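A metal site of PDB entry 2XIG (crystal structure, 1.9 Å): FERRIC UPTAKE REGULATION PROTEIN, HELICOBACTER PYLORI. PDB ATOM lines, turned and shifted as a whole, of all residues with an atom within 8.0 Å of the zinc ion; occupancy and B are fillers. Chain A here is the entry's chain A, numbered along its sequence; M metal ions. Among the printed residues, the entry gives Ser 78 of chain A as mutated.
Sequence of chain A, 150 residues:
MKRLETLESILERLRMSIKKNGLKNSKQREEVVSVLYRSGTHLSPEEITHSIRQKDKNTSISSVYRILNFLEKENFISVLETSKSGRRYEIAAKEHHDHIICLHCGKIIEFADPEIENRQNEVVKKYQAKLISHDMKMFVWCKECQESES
The zinc ion is bound by a ring nitrogen (NE2) of His 42 (2.2 Å).
The zinc ion is bound by a ring nitrogen (NE2) of His 97 (2.2 Å).
The zinc ion is bound by NE2 of His 99, at 2.2 Å.
The zinc ion is bound by OE1 of Glu 90, at 2.3 Å.
The side-chain carboxylate (OE2) of Glu 90 is bound to the zinc ion.
Slightly farther from the zinc ion lies OE2 of Glu 110 (2.6 Å).
Of the 20 residues printed, 5 come within 4 Å of the zinc ion.
A ring nitrogen (NE2) of His 42 sits close to the side-chain carboxylate (OE2) of Glu 110, at 2.9 Å.
The backbone carbonyl oxygen of His 42 is in hydrogen-bond range of the guanidinium group of Arg 88 (3.4 Å).
A ring nitrogen (NE2) of His 97 sits close to the side-chain carboxylate (OE2) of Glu 110 (3.0 Å).
ND1 of His 97 lies within hydrogen-bond range of O of Glu 95 (3.2 Å).
The side-chain amino group (NZ) of Lys 94 lies close to the side-chain carboxylate (OE2) of Glu 90 (2.9 Å).
The backbone carbonyl oxygen (O) of Glu 90 sits at hydrogen-bond distance from the backbone NH (N) of Ser 78, at 3.0 Å.
The side-chain amino group of Lys 94 is in salt-bridge range of the side-chain carboxylate of Glu 110, at 3.3 Å.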
ATOM      1  N   GLY A  40       3.217 -20.521   4.575  1.00  0.00           N
ATOM      2  CA  GLY A  40       2.843 -21.812   4.024  1.00  0.00           C
ATOM      3  C   GLY A  40       1.395 -21.861   3.559  1.00  0.00           C
ATOM      4  O   GLY A  40       0.900 -22.906   3.151  1.00  0.00           O
ATOM      5  N   THR A  41       0.712 -20.715   3.625  1.00  0.00           N
ATOM      6  CA  THR A  41      -0.682 -20.641   3.219  1.00  0.00           C
ATOM      7  C   THR A  41      -0.919 -19.568   2.157  1.00  0.00           C
ATOM      8  O   THR A  41      -0.043 -18.780   1.840  1.00  0.00           O
ATOM      9  CB  THR A  41      -1.605 -20.401   4.435  1.00  0.00           C
ATOM     10  OG1 THR A  41      -1.466 -19.053   4.888  1.00  0.00           O
ATOM     11  CG2 THR A  41      -1.243 -21.353   5.568  1.00  0.00           C
ATOM     12  N   HIS A  42      -2.127 -19.568   1.585  1.00  0.00           N
ATOM     13  CA  HIS A  42      -2.537 -18.520   0.656  1.00  0.00           C
ATOM     14  C   HIS A  42      -3.164 -17.399   1.487  1.00  0.00           C
ATOM     15  O   HIS A  42      -4.086 -17.641   2.262  1.00  0.00           O
ATOM     16  CB  HIS A  42      -3.547 -19.073  -0.348  1.00  0.00           C
ATOM     17  CG  HIS A  42      -3.106 -20.339  -1.009  1.00  0.00           C
ATOM     18  ND1 HIS A  42      -3.043 -21.535  -0.337  1.00  0.00           N
ATOM     19  CD2 HIS A  42      -2.683 -20.597  -2.269  1.00  0.00           C
ATOM     20  CE1 HIS A  42      -2.615 -22.475  -1.145  1.00  0.00           C
ATOM     21  NE2 HIS A  42      -2.388 -21.933  -2.328  1.00  0.00           N
ATOM     22  N   SER A  78       1.177 -15.094  -7.227  1.00  0.00           N
ATOM     23  CA  SER A  78       0.027 -15.547  -7.987  1.00  0.00           C
ATOM     24  C   SER A  78      -1.218 -15.439  -7.123  1.00  0.00           C
ATOM     25  O   SER A  78      -1.132 -15.428  -5.889  1.00  0.00           O
ATOM     26  CB  SER A  78       0.199 -16.977  -8.470  1.00  0.00           C
ATOM     27  OG  SER A  78       0.195 -17.874  -7.382  1.00  0.00           O
ATOM     28  N   VAL A  79      -2.359 -15.357  -7.778  1.00  0.00           N
ATOM     29  CA  VAL A  79      -3.619 -15.205  -7.052  1.00  0.00           C
ATOM     30  C   VAL A  79      -4.546 -16.396  -7.255  1.00  0.00           C
ATOM     31  O   VAL A  79      -4.608 -16.995  -8.332  1.00  0.00           O
ATOM     32  CB  VAL A  79      -4.314 -13.879  -7.412  1.00  0.00           C
ATOM     33  CG1 VAL A  79      -4.518 -13.760  -8.907  1.00  0.00           C
ATOM     34  CG2 VAL A  79      -5.652 -13.761  -6.663  1.00  0.00           C
ATOM     35  N   LEU A  80      -5.234 -16.762  -6.177  1.00  0.00           N
ATOM     36  CA  LEU A  80      -6.258 -17.778  -6.222  1.00  0.00           C
ATOM     37  C   LEU A  80      -7.544 -17.065  -5.805  1.00  0.00           C
ATOM     38  O   LEU A  80      -7.602 -16.480  -4.727  1.00  0.00           O
ATOM     39  CB  LEU A  80      -5.935 -18.899  -5.233  1.00  0.00           C
ATOM     40  CG  LEU A  80      -6.960 -20.023  -5.118  1.00  0.00           C
ATOM     41  CD1 LEU A  80      -6.979 -20.831  -6.396  1.00  0.00           C
ATOM     42  CD2 LEU A  80      -6.662 -20.898  -3.914  1.00  0.00           C
ATOM     43  N   ARG A  88      -6.891 -14.756  -2.644  1.00  0.00           N
ATOM     44  CA  ARG A  88      -5.774 -15.098  -1.784  1.00  0.00           C
ATOM     45  C   ARG A  88      -4.508 -15.215  -2.626  1.00  0.00           C
ATOM     46  O   ARG A  88      -4.574 -15.553  -3.795  1.00  0.00           O
ATOM     47  CB  ARG A  88      -6.040 -16.384  -1.001  1.00  0.00           C
ATOM     48  CG  ARG A  88      -7.116 -16.181   0.067  1.00  0.00           C
ATOM     49  CD  ARG A  88      -7.423 -17.440   0.852  1.00  0.00           C
ATOM     50  NE  ARG A  88      -7.488 -17.139   2.278  1.00  0.00           N
ATOM     51  CZ  ARG A  88      -8.379 -16.322   2.839  1.00  0.00           C
ATOM     52  NH1 ARG A  88      -9.286 -15.723   2.078  1.00  0.00           N
ATOM     53  NH2 ARG A  88      -8.358 -16.111   4.147  1.00  0.00           N
ATOM     54  N   TYR A  89      -3.376 -14.912  -2.014  1.00  0.00           N
ATOM     55  CA  TYR A  89      -2.118 -14.824  -2.748  1.00  0.00           C
ATOM     56  C   TYR A  89      -1.063 -15.779  -2.207  1.00  0.00           C
ATOM     57  O   TYR A  89      -1.064 -16.158  -1.027  1.00  0.00           O
ATOM     58  CB  TYR A  89      -1.585 -13.392  -2.704  1.00  0.00           C
ATOM     59  CG  TYR A  89      -2.447 -12.392  -3.436  1.00  0.00           C
ATOM     60  CD1 TYR A  89      -2.160 -12.019  -4.737  1.00  0.00           C
ATOM     61  CD2 TYR A  89      -3.556 -11.814  -2.818  1.00  0.00           C
ATOM     62  CE1 TYR A  89      -2.939 -11.106  -5.416  1.00  0.00           C
ATOM     63  CE2 TYR A  89      -4.353 -10.900  -3.489  1.00  0.00           C
ATOM     64  CZ  TYR A  89      -4.033 -10.543  -4.787  1.00  0.00           C
ATOM     65  OH  TYR A  89      -4.802  -9.630  -5.470  1.00  0.00           O
ATOM     66  N   GLU A  90      -0.112 -16.135  -3.065  1.00  0.00           N
ATOM     67  CA  GLU A  90       0.992 -16.964  -2.654  1.00  0.00           C
ATOM     68  C   GLU A  90       2.222 -16.622  -3.484  1.00  0.00           C
ATOM     69  O   GLU A  90       2.110 -16.050  -4.572  1.00  0.00           O
ATOM     70  CB  GLU A  90       0.647 -18.446  -2.836  1.00  0.00           C
ATOM     71  CG  GLU A  90       0.355 -18.825  -4.270  1.00  0.00           C
ATOM     72  CD  GLU A  90      -0.132 -20.248  -4.386  1.00  0.00           C
ATOM     73  OE1 GLU A  90      -1.063 -20.506  -5.193  1.00  0.00           O
ATOM     74  OE2 GLU A  90       0.416 -21.115  -3.665  1.00  0.00           O
ATOM     75  N   ILE A  91       3.382 -16.958  -2.954  1.00  0.00           N
ATOM     76  CA  ILE A  91       4.619 -16.745  -3.678  1.00  0.00           C
ATOM     77  C   ILE A  91       4.587 -17.533  -4.990  1.00  0.00           C
ATOM     78  O   ILE A  91       4.112 -18.663  -5.038  1.00  0.00           O
ATOM     79  CB  ILE A  91       5.818 -17.171  -2.820  1.00  0.00           C
ATOM     80  CG1 ILE A  91       7.106 -16.532  -3.353  1.00  0.00           C
ATOM     81  CG2 ILE A  91       5.894 -18.695  -2.730  1.00  0.00           C
ATOM     82  CD1 ILE A  91       7.160 -15.040  -3.114  1.00  0.00           C
ATOM     83  N   LYS A  94       6.950 -21.503  -6.669  1.00  0.00           N
ATOM     84  CA  LYS A  94       6.647 -22.849  -6.191  1.00  0.00           C
ATOM     85  C   LYS A  94       6.349 -23.713  -7.402  1.00  0.00           C
ATOM     86  O   LYS A  94       5.928 -23.209  -8.438  1.00  0.00           O
ATOM     87  CB  LYS A  94       5.431 -22.846  -5.245  1.00  0.00           C
ATOM     88  CG  LYS A  94       5.534 -21.818  -4.129  1.00  0.00           C
ATOM     89  CD  LYS A  94       4.700 -22.204  -2.906  1.00  0.00           C
ATOM     90  CE  LYS A  94       3.214 -22.275  -3.204  1.00  0.00           C
ATOM     91  NZ  LYS A  94       2.408 -22.259  -1.944  1.00  0.00           N
ATOM     92  N   GLU A  95       6.568 -25.016  -7.286  1.00  0.00           N
ATOM     93  CA  GLU A  95       6.280 -25.904  -8.396  1.00  0.00           C
ATOM     94  C   GLU A  95       4.796 -25.809  -8.737  1.00  0.00           C
ATOM     95  O   GLU A  95       3.975 -25.485  -7.875  1.00  0.00           O
ATOM     96  CB  GLU A  95       6.661 -27.352  -8.064  1.00  0.00           C
ATOM     97  CG  GLU A  95       8.167 -27.571  -8.060  1.00  0.00           C
ATOM     98  CD  GLU A  95       8.542 -29.022  -7.894  1.00  0.00           C
ATOM     99  OE1 GLU A  95       9.713 -29.381  -8.194  1.00  0.00           O
ATOM    100  OE2 GLU A  95       7.673 -29.817  -7.458  1.00  0.00           O
ATOM    101  N   HIS A  96       4.458 -26.088  -9.988  1.00  0.00           N
ATOM    102  CA  HIS A  96       3.075 -26.010 -10.420  1.00  0.00           C
ATOM    103  C   HIS A  96       2.164 -26.856  -9.544  1.00  0.00           C
ATOM    104  O   HIS A  96       2.506 -27.971  -9.144  1.00  0.00           O
ATOM    105  CB  HIS A  96       2.914 -26.479 -11.867  1.00  0.00           C
ATOM    106  CG  HIS A  96       1.492 -26.662 -12.257  1.00  0.00           C
ATOM    107  ND1 HIS A  96       0.651 -25.596 -12.519  1.00  0.00           N
ATOM    108  CD2 HIS A  96       0.726 -27.779 -12.349  1.00  0.00           C
ATOM    109  CE1 HIS A  96      -0.559 -26.057 -12.786  1.00  0.00           C
ATOM    110  NE2 HIS A  96      -0.545 -27.376 -12.690  1.00  0.00           N
ATOM    111  N   HIS A  97       0.991 -26.320  -9.248  1.00  0.00           N
ATOM    112  CA  HIS A  97      -0.014 -27.092  -8.547  1.00  0.00           C
ATOM    113  C   HIS A  97      -1.381 -26.505  -8.806  1.00  0.00           C
ATOM    114  O   HIS A  97      -1.502 -25.335  -9.181  1.00  0.00           O
ATOM    115  CB  HIS A  97       0.265 -27.109  -7.043  1.00  0.00           C
ATOM    116  CG  HIS A  97       0.177 -25.768  -6.407  1.00  0.00           C
ATOM    117  ND1 HIS A  97       1.203 -24.847  -6.446  1.00  0.00           N
ATOM    118  CD2 HIS A  97      -0.837 -25.177  -5.724  1.00  0.00           C
ATOM    119  CE1 HIS A  97       0.820 -23.752  -5.803  1.00  0.00           C
ATOM    120  NE2 HIS A  97      -0.399 -23.929  -5.346  1.00  0.00           N
ATOM    121  N   ASP A  98      -2.401 -27.311  -8.590  1.00  0.00           N
ATOM    122  CA  ASP A  98      -3.775 -26.845  -8.724  1.00  0.00           C
ATOM    123  C   ASP A  98      -4.437 -26.855  -7.352  1.00  0.00           C
ATOM    124  O   ASP A  98      -3.808 -27.205  -6.359  1.00  0.00           O
ATOM    125  CB  ASP A  98      -4.516 -27.720  -9.721  1.00  0.00           C
ATOM    126  CG  ASP A  98      -3.790 -27.810 -11.058  1.00  0.00           C
ATOM    127  OD1 ASP A  98      -3.748 -26.801 -11.794  1.00  0.00           O
ATOM    128  OD2 ASP A  98      -3.252 -28.889 -11.368  1.00  0.00           O
ATOM    129  N   HIS A  99      -5.703 -26.452  -7.280  1.00  0.00           N
ATOM    130  CA  HIS A  99      -6.343 -26.263  -5.983  1.00  0.00           C
ATOM    131  C   HIS A  99      -7.680 -26.943  -5.835  1.00  0.00           C
ATOM    132  O   HIS A  99      -8.504 -26.937  -6.733  1.00  0.00           O
ATOM    133  CB  HIS A  99      -6.529 -24.772  -5.667  1.00  0.00           C
ATOM    134  CG  HIS A  99      -5.258 -23.998  -5.727  1.00  0.00           C
ATOM    135  ND1 HIS A  99      -4.756 -23.490  -6.900  1.00  0.00           N
ATOM    136  CD2 HIS A  99      -4.364 -23.667  -4.761  1.00  0.00           C
ATOM    137  CE1 HIS A  99      -3.618 -22.865  -6.668  1.00  0.00           C
ATOM    138  NE2 HIS A  99      -3.356 -22.958  -5.369  1.00  0.00           N
ATOM    139  N   ILE A 108      -8.248 -24.690   1.721  1.00  0.00           N
ATOM    140  CA  ILE A 108      -7.586 -24.904   0.430  1.00  0.00           C
ATOM    141  C   ILE A 108      -6.607 -26.072   0.494  1.00  0.00           C
ATOM    142  O   ILE A 108      -5.785 -26.150   1.395  1.00  0.00           O
ATOM    143  CB  ILE A 108      -6.822 -23.638  -0.006  1.00  0.00           C
ATOM    144  CG1 ILE A 108      -7.775 -22.448  -0.140  1.00  0.00           C
ATOM    145  CG2 ILE A 108      -6.074 -23.869  -1.325  1.00  0.00           C
ATOM    146  CD1 ILE A 108      -7.078 -21.082  -0.138  1.00  0.00           C
ATOM    147  N   ILE A 109      -6.720 -27.002  -0.456  1.00  0.00           N
ATOM    148  CA  ILE A 109      -5.799 -28.124  -0.557  1.00  0.00           C
ATOM    149  C   ILE A 109      -5.047 -28.081  -1.901  1.00  0.00           C
ATOM    150  O   ILE A 109      -5.659 -27.980  -2.951  1.00  0.00           O
ATOM    151  CB  ILE A 109      -6.541 -29.469  -0.389  1.00  0.00           C
ATOM    152  CG1 ILE A 109      -7.152 -29.577   1.012  1.00  0.00           C
ATOM    153  CG2 ILE A 109      -5.613 -30.623  -0.671  1.00  0.00           C
ATOM    154  CD1 ILE A 109      -7.991 -30.812   1.219  1.00  0.00           C
ATOM    155  N   GLU A 110      -3.719 -28.127  -1.852  1.00  0.00           N
ATOM    156  CA  GLU A 110      -2.925 -28.098  -3.071  1.00  0.00           C
ATOM    157  C   GLU A 110      -2.689 -29.505  -3.609  1.00  0.00           C
ATOM    158  O   GLU A 110      -2.572 -30.451  -2.842  1.00  0.00           O
ATOM    159  CB  GLU A 110      -1.585 -27.396  -2.811  1.00  0.00           C
ATOM    160  CG  GLU A 110      -1.742 -25.959  -2.321  1.00  0.00           C
ATOM    161  CD  GLU A 110      -0.427 -25.240  -2.169  1.00  0.00           C
ATOM    162  OE1 GLU A 110       0.580 -25.899  -1.803  1.00  0.00           O
ATOM    163  OE2 GLU A 110      -0.404 -24.011  -2.397  1.00  0.00           O
ATOM    164  N   PHE A 111      -2.646 -29.639  -4.932  1.00  0.00           N
ATOM    165  CA  PHE A 111      -2.352 -30.933  -5.550  1.00  0.00           C
ATOM    166  C   PHE A 111      -1.731 -30.753  -6.912  1.00  0.00           C
ATOM    167  O   PHE A 111      -1.891 -29.711  -7.565  1.00  0.00           O
ATOM    168  CB  PHE A 111      -3.618 -31.808  -5.644  1.00  0.00           C
ATOM    169  CG  PHE A 111      -4.601 -31.368  -6.710  1.00  0.00           C
ATOM    170  CD1 PHE A 111      -5.546 -30.382  -6.447  1.00  0.00           C
ATOM    171  CD2 PHE A 111      -4.581 -31.935  -7.981  1.00  0.00           C
ATOM    172  CE1 PHE A 111      -6.457 -29.974  -7.419  1.00  0.00           C
ATOM    173  CE2 PHE A 111      -5.475 -31.538  -8.962  1.00  0.00           C
ATOM    174  CZ  PHE A 111      -6.422 -30.557  -8.677  1.00  0.00           C
HETATM  175 ZN    ZN M   1      -1.550 -22.493  -4.228  1.00  0.00          ZN
